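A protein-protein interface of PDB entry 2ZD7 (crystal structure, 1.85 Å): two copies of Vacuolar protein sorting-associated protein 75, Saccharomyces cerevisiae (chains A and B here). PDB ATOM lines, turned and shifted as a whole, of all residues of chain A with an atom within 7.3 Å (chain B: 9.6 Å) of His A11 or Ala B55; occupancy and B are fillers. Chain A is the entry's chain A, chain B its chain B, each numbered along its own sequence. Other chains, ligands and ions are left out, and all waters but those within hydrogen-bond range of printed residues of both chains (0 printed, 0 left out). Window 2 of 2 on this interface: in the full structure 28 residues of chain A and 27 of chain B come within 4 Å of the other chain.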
ATOM      1  N   GLU A   6      -9.854 -16.024   0.242  1.00  0.00           N
ATOM      2  CA  GLU A   6     -10.768 -16.772   1.097  1.00  0.00           C
ATOM      3  C   GLU A   6     -10.064 -17.227   2.371  1.00  0.00           C
ATOM      4  O   GLU A   6     -10.646 -17.211   3.455  1.00  0.00           O
ATOM      5  CB  GLU A   6     -11.308 -17.990   0.349  1.00  0.00           C
ATOM      6  CG  GLU A   6     -12.035 -17.650  -0.939  1.00  0.00           C
ATOM      7  CD  GLU A   6     -12.569 -18.880  -1.646  1.00  0.00           C
ATOM      8  OE1 GLU A   6     -13.435 -19.571  -1.068  1.00  0.00           O
ATOM      9  OE2 GLU A   6     -12.120 -19.156  -2.779  1.00  0.00           O
ATOM     10  N   ASN A   7      -8.806 -17.631   2.232  1.00  0.00           N
ATOM     11  CA  ASN A   7      -8.018 -18.092   3.367  1.00  0.00           C
ATOM     12  C   ASN A   7      -7.604 -16.933   4.270  1.00  0.00           C
ATOM     13  O   ASN A   7      -7.772 -17.002   5.489  1.00  0.00           O
ATOM     14  CB  ASN A   7      -6.780 -18.845   2.872  1.00  0.00           C
ATOM     15  CG  ASN A   7      -7.137 -20.113   2.116  1.00  0.00           C
ATOM     16  OD1 ASN A   7      -7.709 -21.049   2.681  1.00  0.00           O
ATOM     17  ND2 ASN A   7      -6.804 -20.148   0.827  1.00  0.00           N
ATOM     18  N   GLU A   8      -7.066 -15.869   3.677  1.00  0.00           N
ATOM     19  CA  GLU A   8      -6.652 -14.708   4.458  1.00  0.00           C
ATOM     20  C   GLU A   8      -7.872 -14.129   5.167  1.00  0.00           C
ATOM     21  O   GLU A   8      -7.751 -13.469   6.200  1.00  0.00           O
ATOM     22  CB  GLU A   8      -6.016 -13.646   3.555  1.00  0.00           C
ATOM     23  CG  GLU A   8      -4.754 -14.112   2.840  1.00  0.00           C
ATOM     24  CD  GLU A   8      -4.060 -12.991   2.089  1.00  0.00           C
ATOM     25  OE1 GLU A   8      -4.722 -12.333   1.260  1.00  0.00           O
ATOM     26  OE2 GLU A   8      -2.852 -12.771   2.323  1.00  0.00           O
ATOM     27  N   ASN A   9      -9.048 -14.387   4.603  1.00  0.00           N
ATOM     28  CA  ASN A   9     -10.295 -13.915   5.187  1.00  0.00           C
ATOM     29  C   ASN A   9     -10.627 -14.855   6.342  1.00  0.00           C
ATOM     30  O   ASN A   9     -11.123 -14.427   7.386  1.00  0.00           O
ATOM     31  CB  ASN A   9     -11.415 -13.947   4.145  1.00  0.00           C
ATOM     32  CG  ASN A   9     -12.587 -13.057   4.520  1.00  0.00           C
ATOM     33  OD1 ASN A   9     -12.450 -11.834   4.610  1.00  0.00           O
ATOM     34  ND2 ASN A   9     -13.747 -13.666   4.741  1.00  0.00           N
ATOM     35  N   GLU A  10     -10.351 -16.142   6.142  1.00  0.00           N
ATOM     36  CA  GLU A  10     -10.589 -17.156   7.166  1.00  0.00           C
ATOM     37  C   GLU A  10      -9.663 -16.905   8.350  1.00  0.00           C
ATOM     38  O   GLU A  10     -10.066 -17.044   9.505  1.00  0.00           O
ATOM     39  CB  GLU A  10     -10.338 -18.558   6.606  1.00  0.00           C
ATOM     40  CG  GLU A  10     -11.415 -19.044   5.657  1.00  0.00           C
ATOM     41  CD  GLU A  10     -12.757 -19.205   6.344  1.00  0.00           C
ATOM     42  OE1 GLU A  10     -12.836 -19.997   7.308  1.00  0.00           O
ATOM     43  OE2 GLU A  10     -13.731 -18.541   5.922  1.00  0.00           O
ATOM     44  N   HIS A  11      -8.419 -16.540   8.057  1.00  0.00           N
ATOM     45  CA  HIS A  11      -7.449 -16.253   9.103  1.00  0.00           C
ATOM     46  C   HIS A  11      -7.867 -14.998   9.857  1.00  0.00           C
ATOM     47  O   HIS A  11      -7.720 -14.919  11.078  1.00  0.00           O
ATOM     48  CB  HIS A  11      -6.053 -16.061   8.506  1.00  0.00           C
ATOM     49  CG  HIS A  11      -5.257 -17.326   8.410  1.00  0.00           C
ATOM     50  ND1 HIS A  11      -5.730 -18.460   7.785  1.00  0.00           N
ATOM     51  CD2 HIS A  11      -4.015 -17.632   8.855  1.00  0.00           C
ATOM     52  CE1 HIS A  11      -4.813 -19.410   7.848  1.00  0.00           C
ATOM     53  NE2 HIS A  11      -3.762 -18.933   8.491  1.00  0.00           N
ATOM     54  N   ALA A  12      -8.387 -14.015   9.125  1.00  0.00           N
ATOM     55  CA  ALA A  12      -8.834 -12.771   9.739  1.00  0.00           C
ATOM     56  C   ALA A  12     -10.017 -13.073  10.651  1.00  0.00           C
ATOM     57  O   ALA A  12     -10.063 -12.603  11.790  1.00  0.00           O
ATOM     58  CB  ALA A  12      -9.234 -11.770   8.668  1.00  0.00           C
ATOM     59  N   LYS A  13     -10.971 -13.853  10.147  1.00  0.00           N
ATOM     60  CA  LYS A  13     -12.144 -14.229  10.932  1.00  0.00           C
ATOM     61  C   LYS A  13     -11.676 -14.944  12.194  1.00  0.00           C
ATOM     62  O   LYS A  13     -12.177 -14.692  13.288  1.00  0.00           O
ATOM     63  CB  LYS A  13     -13.054 -15.181  10.148  1.00  0.00           C
ATOM     64  CG  LYS A  13     -13.761 -14.578   8.945  1.00  0.00           C
ATOM     65  CD  LYS A  13     -14.677 -15.608   8.297  1.00  0.00           C
ATOM     66  CE  LYS A  13     -15.455 -15.021   7.125  1.00  0.00           C
ATOM     67  NZ  LYS A  13     -16.359 -16.040   6.521  1.00  0.00           N
ATOM     68  N   ALA A  14     -10.710 -15.844  12.021  1.00  0.00           N
ATOM     69  CA  ALA A  14     -10.161 -16.616  13.130  1.00  0.00           C
ATOM     70  C   ALA A  14      -9.530 -15.710  14.180  1.00  0.00           C
ATOM     71  O   ALA A  14      -9.818 -15.842  15.369  1.00  0.00           O
ATOM     72  CB  ALA A  14      -9.131 -17.615  12.610  1.00  0.00           C
ATOM     73  N   PHE A  15      -8.672 -14.795  13.738  1.00  0.00           N
ATOM     74  CA  PHE A  15      -8.005 -13.867  14.642  1.00  0.00           C
ATOM     75  C   PHE A  15      -9.010 -13.013  15.406  1.00  0.00           C
ATOM     76  O   PHE A  15      -8.837 -12.756  16.598  1.00  0.00           O
ATOM     77  CB  PHE A  15      -7.041 -12.963  13.870  1.00  0.00           C
ATOM     78  CG  PHE A  15      -5.807 -13.670  13.367  1.00  0.00           C
ATOM     79  CD1 PHE A  15      -4.801 -12.957  12.726  1.00  0.00           C
ATOM     80  CD2 PHE A  15      -5.647 -15.043  13.536  1.00  0.00           C
ATOM     81  CE1 PHE A  15      -3.651 -13.597  12.259  1.00  0.00           C
ATOM     82  CE2 PHE A  15      -4.506 -15.692  13.074  1.00  0.00           C
ATOM     83  CZ  PHE A  15      -3.506 -14.967  12.433  1.00  0.00           C
ATOM     84  N   LEU A  16     -10.059 -12.569  14.721  1.00  0.00           N
ATOM     85  CA  LEU A  16     -11.081 -11.762  15.373  1.00  0.00           C
ATOM     86  C   LEU A  16     -11.784 -12.633  16.405  1.00  0.00           C
ATOM     87  O   LEU A  16     -12.076 -12.189  17.517  1.00  0.00           O
ATOM     88  CB  LEU A  16     -12.102 -11.249  14.352  1.00  0.00           C
ATOM     89  CG  LEU A  16     -11.593 -10.239  13.320  1.00  0.00           C
ATOM     90  CD1 LEU A  16     -12.725  -9.870  12.363  1.00  0.00           C
ATOM     91  CD2 LEU A  16     -11.057  -9.001  14.033  1.00  0.00           C
ATOM     92  N   GLY A  17     -12.042 -13.881  16.029  1.00  0.00           N
ATOM     93  CA  GLY A  17     -12.709 -14.800  16.928  1.00  0.00           C
ATOM     94  C   GLY A  17     -11.889 -15.077  18.175  1.00  0.00           C
ATOM     95  O   GLY A  17     -12.421 -15.109  19.287  1.00  0.00           O
ATOM     96  N   LEU A  18     -10.588 -15.266  17.985  1.00  0.00           N
ATOM     97  CA  LEU A  18      -9.678 -15.546  19.089  1.00  0.00           C
ATOM     98  C   LEU A  18      -9.561 -14.355  20.028  1.00  0.00           C
ATOM     99  O   LEU A  18      -9.507 -14.525  21.244  1.00  0.00           O
ATOM    100  CB  LEU A  18      -8.295 -15.921  18.555  1.00  0.00           C
ATOM    101  CG  LEU A  18      -8.210 -17.215  17.741  1.00  0.00           C
ATOM    102  CD1 LEU A  18      -6.762 -17.474  17.368  1.00  0.00           C
ATOM    103  CD2 LEU A  18      -8.769 -18.384  18.551  1.00  0.00           C
ATOM    104  N   ALA B  49     -12.484 -23.993  17.854  1.00  0.00           N
ATOM    105  CA  ALA B  49     -13.118 -23.998  16.531  1.00  0.00           C
ATOM    106  C   ALA B  49     -12.418 -22.982  15.621  1.00  0.00           C
ATOM    107  O   ALA B  49     -12.232 -23.228  14.428  1.00  0.00           O
ATOM    108  CB  ALA B  49     -14.600 -23.664  16.655  1.00  0.00           C
ATOM    109  N   TYR B  50     -12.026 -21.844  16.189  1.00  0.00           N
ATOM    110  CA  TYR B  50     -11.320 -20.808  15.436  1.00  0.00           C
ATOM    111  C   TYR B  50      -9.894 -21.270  15.144  1.00  0.00           C
ATOM    112  O   TYR B  50      -9.357 -21.026  14.059  1.00  0.00           O
ATOM    113  CB  TYR B  50     -11.261 -19.504  16.233  1.00  0.00           C
ATOM    114  CG  TYR B  50     -12.576 -18.774  16.342  1.00  0.00           C
ATOM    115  CD1 TYR B  50     -13.108 -18.447  17.585  1.00  0.00           C
ATOM    116  CD2 TYR B  50     -13.275 -18.375  15.199  1.00  0.00           C
ATOM    117  CE1 TYR B  50     -14.300 -17.735  17.697  1.00  0.00           C
ATOM    118  CE2 TYR B  50     -14.469 -17.666  15.300  1.00  0.00           C
ATOM    119  CZ  TYR B  50     -14.972 -17.348  16.550  1.00  0.00           C
ATOM    120  OH  TYR B  50     -16.133 -16.618  16.664  1.00  0.00           O
ATOM    121  N   ILE B  51      -9.281 -21.928  16.127  1.00  0.00           N
ATOM    122  CA  ILE B  51      -7.923 -22.441  15.975  1.00  0.00           C
ATOM    123  C   ILE B  51      -7.867 -23.427  14.808  1.00  0.00           C
ATOM    124  O   ILE B  51      -6.908 -23.434  14.036  1.00  0.00           O
ATOM    125  CB  ILE B  51      -7.454 -23.164  17.267  1.00  0.00           C
ATOM    126  CG1 ILE B  51      -7.207 -22.142  18.379  1.00  0.00           C
ATOM    127  CG2 ILE B  51      -6.192 -23.968  16.995  1.00  0.00           C
ATOM    128  CD1 ILE B  51      -6.841 -22.778  19.732  1.00  0.00           C
ATOM    129  N   ASP B  52      -8.900 -24.253  14.684  1.00  0.00           N
ATOM    130  CA  ASP B  52      -8.968 -25.245  13.616  1.00  0.00           C
ATOM    131  C   ASP B  52      -8.960 -24.615  12.227  1.00  0.00           C
ATOM    132  O   ASP B  52      -8.768 -25.308  11.226  1.00  0.00           O
ATOM    133  CB  ASP B  52     -10.219 -26.115  13.764  1.00  0.00           C
ATOM    134  CG  ASP B  52     -10.185 -26.988  15.005  1.00  0.00           C
ATOM    135  OD1 ASP B  52      -9.088 -27.474  15.364  1.00  0.00           O
ATOM    136  OD2 ASP B  52     -11.255 -27.201  15.614  1.00  0.00           O
ATOM    137  N   GLU B  53      -9.169 -23.303  12.170  1.00  0.00           N
ATOM    138  CA  GLU B  53      -9.186 -22.583  10.904  1.00  0.00           C
ATOM    139  C   GLU B  53      -7.820 -22.002  10.559  1.00  0.00           C
ATOM    140  O   GLU B  53      -7.636 -21.445   9.476  1.00  0.00           O
ATOM    141  CB  GLU B  53     -10.215 -21.448  10.953  1.00  0.00           C
ATOM    142  CG  GLU B  53     -11.663 -21.901  10.944  1.00  0.00           C
ATOM    143  CD  GLU B  53     -12.631 -20.753  11.188  1.00  0.00           C
ATOM    144  OE1 GLU B  53     -12.498 -19.705  10.517  1.00  0.00           O
ATOM    145  OE2 GLU B  53     -13.527 -20.901  12.049  1.00  0.00           O
ATOM    146  N   ILE B  54      -6.865 -22.128  11.476  1.00  0.00           N
ATOM    147  CA  ILE B  54      -5.525 -21.599  11.249  1.00  0.00           C
ATOM    148  C   ILE B  54      -4.519 -22.691  10.894  1.00  0.00           C
ATOM    149  O   ILE B  54      -4.168 -23.527  11.726  1.00  0.00           O
ATOM    150  CB  ILE B  54      -5.016 -20.828  12.478  1.00  0.00           C
ATOM    151  CG1 ILE B  54      -5.947 -19.651  12.772  1.00  0.00           C
ATOM    152  CG2 ILE B  54      -3.604 -20.325  12.228  1.00  0.00           C
ATOM    153  CD1 ILE B  54      -5.531 -18.823  13.974  1.00  0.00           C
ATOM    154  N   ALA B  55      -4.063 -22.652   9.645  1.00  0.00           N
ATOM    155  CA  ALA B  55      -3.107 -23.605   9.088  1.00  0.00           C
ATOM    156  C   ALA B  55      -2.186 -24.334  10.064  1.00  0.00           C
ATOM    157  O   ALA B  55      -2.561 -25.348  10.661  1.00  0.00           O
ATOM    158  CB  ALA B  55      -2.259 -22.908   8.019  1.00  0.00           C
ATOM    159  N   GLU B  56      -0.973 -23.812  10.204  1.00  0.00           N
ATOM    160  CA  GLU B  56       0.044 -24.405  11.062  1.00  0.00           C
ATOM    161  C   GLU B  56       0.024 -23.877  12.491  1.00  0.00           C
ATOM    162  O   GLU B  56       1.076 -23.659  13.083  1.00  0.00           O
ATOM    163  CB  GLU B  56       1.427 -24.145  10.463  1.00  0.00           C
ATOM    164  CG  GLU B  56       1.594 -24.593   9.022  1.00  0.00           C
ATOM    165  CD  GLU B  56       2.961 -24.233   8.468  1.00  0.00           C
ATOM    166  OE1 GLU B  56       3.280 -23.026   8.413  1.00  0.00           O
ATOM    167  OE2 GLU B  56       3.718 -25.155   8.093  1.00  0.00           O
ATOM    168  N   PHE B  57      -1.159 -23.681  13.052  1.00  0.00           N
ATOM    169  CA  PHE B  57      -1.253 -23.161  14.409  1.00  0.00           C
ATOM    170  C   PHE B  57      -0.415 -23.948  15.422  1.00  0.00           C
ATOM    171  O   PHE B  57       0.516 -23.406  16.013  1.00  0.00           O
ATOM    172  CB  PHE B  57      -2.704 -23.147  14.875  1.00  0.00           C
ATOM    173  CG  PHE B  57      -2.892 -22.517  16.225  1.00  0.00           C
ATOM    174  CD1 PHE B  57      -2.968 -21.133  16.359  1.00  0.00           C
ATOM    175  CD2 PHE B  57      -2.995 -23.309  17.366  1.00  0.00           C
ATOM    176  CE1 PHE B  57      -3.150 -20.542  17.613  1.00  0.00           C
ATOM    177  CE2 PHE B  57      -3.176 -22.728  18.623  1.00  0.00           C
ATOM    178  CZ  PHE B  57      -3.255 -21.345  18.745  1.00  0.00           C
ATOM    179  N   TRP B  58      -0.747 -25.221  15.621  1.00  0.00           N
ATOM    180  CA  TRP B  58      -0.016 -26.037  16.591  1.00  0.00           C
ATOM    181  C   TRP B  58       1.454 -26.233  16.234  1.00  0.00           C
ATOM    182  O   TRP B  58       2.302 -26.352  17.118  1.00  0.00           O
ATOM    183  CB  TRP B  58      -0.715 -27.382  16.788  1.00  0.00           C
ATOM    184  CG  TRP B  58      -2.056 -27.238  17.447  1.00  0.00           C
ATOM    185  CD1 TRP B  58      -3.274 -27.486  16.890  1.00  0.00           C
ATOM    186  CD2 TRP B  58      -2.313 -26.775  18.783  1.00  0.00           C
ATOM    187  NE1 TRP B  58      -4.276 -27.204  17.790  1.00  0.00           N
ATOM    188  CE2 TRP B  58      -3.713 -26.767  18.961  1.00  0.00           C
ATOM    189  CE3 TRP B  58      -1.494 -26.366  19.845  1.00  0.00           C
ATOM    190  CZ2 TRP B  58      -4.317 -26.364  20.159  1.00  0.00           C
ATOM    191  CZ3 TRP B  58      -2.093 -25.966  21.039  1.00  0.00           C
ATOM    192  CH2 TRP B  58      -3.492 -25.969  21.186  1.00  0.00           C
ATOM    193  N   LYS B  59       1.763 -26.253  14.943  1.00  0.00           N
ATOM    194  CA  LYS B  59       3.150 -26.403  14.520  1.00  0.00           C
ATOM    195  C   LYS B  59       3.921 -25.204  15.056  1.00  0.00           C
ATOM    196  O   LYS B  59       4.996 -25.342  15.630  1.00  0.00           O
ATOM    197  CB  LYS B  59       3.241 -26.425  12.996  1.00  0.00           C
ATOM    198  CG  LYS B  59       4.660 -26.367  12.465  1.00  0.00           C
ATOM    199  CD  LYS B  59       4.675 -26.320  10.944  1.00  0.00           C
ATOM    200  CE  LYS B  59       6.087 -26.140  10.413  1.00  0.00           C
ATOM    201  NZ  LYS B  59       6.113 -26.096   8.925  1.00  0.00           N
ATOM    202  N   ILE B  60       3.340 -24.024  14.879  1.00  0.00           N
ATOM    203  CA  ILE B  60       3.955 -22.778  15.319  1.00  0.00           C
ATOM    204  C   ILE B  60       4.036 -22.654  16.840  1.00  0.00           C
ATOM    205  O   ILE B  60       5.051 -22.208  17.384  1.00  0.00           O
ATOM    206  CB  ILE B  60       3.174 -21.572  14.740  1.00  0.00           C
ATOM    207  CG1 ILE B  60       3.174 -21.660  13.210  1.00  0.00           C
ATOM    208  CG2 ILE B  60       3.801 -20.268  15.196  1.00  0.00           C
ATOM    209  CD1 ILE B  60       2.446 -20.530  12.519  1.00  0.00           C
ATOM    210  N   VAL B  61       2.962 -23.042  17.522  1.00  0.00           N
ATOM    211  CA  VAL B  61       2.917 -22.973  18.979  1.00  0.00           C
ATOM    212  C   VAL B  61       3.962 -23.884  19.631  1.00  0.00           C
ATOM    213  O   VAL B  61       4.743 -23.440  20.474  1.00  0.00           O
ATOM    214  CB  VAL B  61       1.512 -23.356  19.498  1.00  0.00           C
ATOM    215  CG1 VAL B  61       1.520 -23.496  21.016  1.00  0.00           C
ATOM    216  CG2 VAL B  61       0.504 -22.287  19.079  1.00  0.00           C
ATOM    217  N   ASP B  81       5.410 -31.386  13.837  1.00  0.00           N
ATOM    218  CA  ASP B  81       4.921 -30.365  12.912  1.00  0.00           C
ATOM    219  C   ASP B  81       3.626 -30.768  12.215  1.00  0.00           C
ATOM    220  O   ASP B  81       2.950 -29.925  11.624  1.00  0.00           O
ATOM    221  CB  ASP B  81       5.975 -30.052  11.843  1.00  0.00           C
ATOM    222  CG  ASP B  81       7.125 -29.214  12.371  1.00  0.00           C
ATOM    223  OD1 ASP B  81       7.019 -28.660  13.487  1.00  0.00           O
ATOM    224  OD2 ASP B  81       8.141 -29.096  11.653  1.00  0.00           O
ATOM    225  N   THR B  82       3.280 -32.048  12.285  1.00  0.00           N
ATOM    226  CA  THR B  82       2.067 -32.543  11.642  1.00  0.00           C
ATOM    227  C   THR B  82       0.839 -32.510  12.557  1.00  0.00           C
ATOM    228  O   THR B  82      -0.267 -32.868  12.149  1.00  0.00           O
ATOM    229  CB  THR B  82       2.269 -33.979  11.128  1.00  0.00           C
ATOM    230  OG1 THR B  82       1.279 -34.270  10.138  1.00  0.00           O
ATOM    231  CG2 THR B  82       2.126 -34.979  12.253  1.00  0.00           C
ATOM    232  N   ILE B  83       1.036 -32.087  13.799  1.00  0.00           N
ATOM    233  CA  ILE B  83      -0.066 -31.994  14.747  1.00  0.00           C
ATOM    234  C   ILE B  83      -1.011 -30.888  14.270  1.00  0.00           C
ATOM    235  O   ILE B  83      -0.601 -29.734  14.169  1.00  0.00           O
ATOM    236  CB  ILE B  83       0.456 -31.652  16.169  1.00  0.00           C
ATOM    237  CG1 ILE B  83       1.263 -32.835  16.722  1.00  0.00           C
ATOM    238  CG2 ILE B  83      -0.715 -31.303  17.083  1.00  0.00           C
ATOM    239  CD1 ILE B  83       1.809 -32.626  18.140  1.00  0.00           C
ATOM    240  N   ASP B  84      -2.261 -31.250  13.983  1.00  0.00           N
ATOM    241  CA  ASP B  84      -3.280 -30.309  13.494  1.00  0.00           C
ATOM    242  C   ASP B  84      -4.322 -29.961  14.534  1.00  0.00           C
ATOM    243  O   ASP B  84      -5.155 -29.081  14.310  1.00  0.00           O
ATOM    244  CB  ASP B  84      -4.061 -30.889  12.305  1.00  0.00           C
ATOM    245  CG  ASP B  84      -3.200 -31.173  11.109  1.00  0.00           C
ATOM    246  OD1 ASP B  84      -2.189 -30.467  10.910  1.00  0.00           O
ATOM    247  OD2 ASP B  84      -3.554 -32.099  10.354  1.00  0.00           O
ATOM    248  N   LYS B  85      -4.323 -30.680  15.645  1.00  0.00           N
ATOM    249  CA  LYS B  85      -5.306 -30.417  16.678  1.00  0.00           C
ATOM    250  C   LYS B  85      -4.920 -31.020  18.018  1.00  0.00           C
ATOM    251  O   LYS B  85      -4.415 -32.142  18.102  1.00  0.00           O
ATOM    252  CB  LYS B  85      -6.670 -30.962  16.252  1.00  0.00           C
ATOM    253  CG  LYS B  85      -7.815 -30.629  17.199  1.00  0.00           C
ATOM    254  CD  LYS B  85      -9.146 -31.148  16.656  1.00  0.00           C
ATOM    255  CE  LYS B  85     -10.287 -30.862  17.625  1.00  0.00           C
ATOM    256  NZ  LYS B  85     -10.463 -29.399  17.883  1.00  0.00           N
ATOM    257  N   HIS B 108      -4.152 -34.929  16.995  1.00  0.00           N
ATOM    258  CA  HIS B 108      -4.429 -35.413  15.650  1.00  0.00           C
ATOM    259  C   HIS B 108      -3.191 -35.093  14.828  1.00  0.00           C
ATOM    260  O   HIS B 108      -2.756 -33.944  14.756  1.00  0.00           O
ATOM    261  CB  HIS B 108      -5.652 -34.760  15.001  1.00  0.00           C
ATOM    262  CG  HIS B 108      -5.912 -35.266  13.613  1.00  0.00           C
ATOM    263  ND1 HIS B 108      -5.362 -34.682  12.493  1.00  0.00           N
ATOM    264  CD2 HIS B 108      -6.559 -36.376  13.178  1.00  0.00           C
ATOM    265  CE1 HIS B 108      -5.651 -35.411  11.428  1.00  0.00           C
ATOM    266  NE2 HIS B 108      -6.375 -36.444  11.817  1.00  0.00           N
ATOM    267  N   HIS B 110      -1.498 -35.139  11.125  1.00  0.00           N
ATOM    268  CA  HIS B 110      -1.876 -35.169   9.714  1.00  0.00           C
ATOM    269  C   HIS B 110      -1.052 -36.247   9.025  1.00  0.00           C
ATOM    270  O   HIS B 110      -1.444 -36.781   7.986  1.00  0.00           O
ATOM    271  CB  HIS B 110      -1.614 -33.801   9.067  1.00  0.00           C
ATOM    272  CG  HIS B 110      -1.794 -33.786   7.579  1.00  0.00           C
ATOM    273  ND1 HIS B 110      -0.814 -34.209   6.706  1.00  0.00           N
ATOM    274  CD2 HIS B 110      -2.845 -33.411   6.811  1.00  0.00           C
ATOM    275  CE1 HIS B 110      -1.254 -34.094   5.464  1.00  0.00           C
ATOM    276  NE2 HIS B 110      -2.484 -33.612   5.501  1.00  0.00           N
ATOM    277  N   TYR B 216       1.165 -18.190  19.980  1.00  0.00           N
ATOM    278  CA  TYR B 216       1.039 -17.918  18.552  1.00  0.00           C
ATOM    279  C   TYR B 216       1.318 -16.445  18.253  1.00  0.00           C
ATOM    280  O   TYR B 216       2.054 -16.113  17.322  1.00  0.00           O
ATOM    281  CB  TYR B 216      -0.363 -18.275  18.061  1.00  0.00           C
ATOM    282  CG  TYR B 216      -0.505 -18.143  16.567  1.00  0.00           C
ATOM    283  CD1 TYR B 216       0.109 -19.052  15.710  1.00  0.00           C
ATOM    284  CD2 TYR B 216      -1.218 -17.084  16.005  1.00  0.00           C
ATOM    285  CE1 TYR B 216       0.023 -18.911  14.330  1.00  0.00           C
ATOM    286  CE2 TYR B 216      -1.308 -16.931  14.620  1.00  0.00           C
ATOM    287  CZ  TYR B 216      -0.684 -17.850  13.790  1.00  0.00           C
ATOM    288  OH  TYR B 216      -0.766 -17.710  12.424  1.00  0.00           O
ATOM    289  N   GLN B 220       4.555 -14.548  15.957  1.00  0.00           N
ATOM    290  CA  GLN B 220       4.459 -13.561  14.892  1.00  0.00           C
ATOM    291  C   GLN B 220       5.214 -12.312  15.332  1.00  0.00           C
ATOM    292  O   GLN B 220       5.920 -11.689  14.543  1.00  0.00           O
ATOM    293  CB  GLN B 220       2.992 -13.242  14.604  1.00  0.00           C
ATOM    294  CG  GLN B 220       2.216 -14.448  14.092  1.00  0.00           C
ATOM    295  CD  GLN B 220       0.801 -14.105  13.669  1.00  0.00           C
ATOM    296  OE1 GLN B 220      -0.007 -13.636  14.473  1.00  0.00           O
ATOM    297  NE2 GLN B 220       0.490 -14.344  12.397  1.00  0.00           N
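OE1 of Glu B53 lies close to OE1 of Glu A10 (3.2 Å).
ND1 of His A11 sits at hydrogen-bond distance from O of Asn A7, 3.4 Å away. The side-chain amino group of Lys A13 lies within salt-bridge range of the side-chain carboxylate of Glu A10, 3.7 Å away.
Among the printed residues, merely in contact across the chains: His A11 with Glu B53 (3.8 Å), His A11 with Ile B54 (3.99 Å), His A11 with Ala B55 (3.8 Å), Ala A14 with Tyr B50 (3.7 Å), Ala A14 with Ile B54 (3.8 Å), Phe A15 with Ile B54 (3.4 Å), Phe A15 with Tyr B216 (3.7 Å), Gly A17 with Tyr B50 (3.4 Å), Leu A18 with Tyr B50 (3.6 Å) and Leu A18 with Ile B54 (3.9 Å).
Printed residues of chain B within 4 Å of Glu A10: Glu B53. Of the printed residues of chain B, His A11 touches Glu B53, Ile B54 and Ala B55. No residue of chain B comes within 4 Å of Ala A12. Printed residues of chain B within 4 Å of Ala A14: Tyr B50 (3.7 Å) and Ile B54 (3.8 Å). Printed residues of chain B within 4 Å of Phe A15: Ile B54 (3.4 Å) and Tyr B216 (3.7 Å). Of the printed residues of chain A, Glu B53 touches Glu A10 and His A11. Ala B55 touches just one residue of chain A: His A11 (3.8 Å). Ile B60 touches none of the printed residues of chain A. Printed residues of chain A within 4 Å of Tyr B216: Phe A15 (3.7 Å). The nearest printed residue of chain A that does not touch Ala B55 is Ala A14 (7.7 Å).
Of the 13 printed residues of chain A, 6 touch a printed residue of chain B. Printed residues of chain A that touch a printed residue of chain B: Glu A10, His A11, Ala A14, Phe A15, Gly A17 and Leu A18. Hydrophobic or aromatic side chains of chain A that line the printed part of chain B: His A11, Ala A14, Phe A15 and Leu A18. Along chain A the printed residues that touch a printed residue of chain B span positions 10 to 18. Of the 22 printed residues of chain B, 5 touch a printed residue of chain A. Hydrophobic or aromatic side chains of chain B that line the printed part of chain A: Tyr B50, Ile B54 and Tyr B216. Among the printed residues, 11 pairs touch across the chains.
No position is printed for both chains. Of the 11 pairs that touch across the chains among the printed residues, none has its exchanged pair printed and touching as well.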
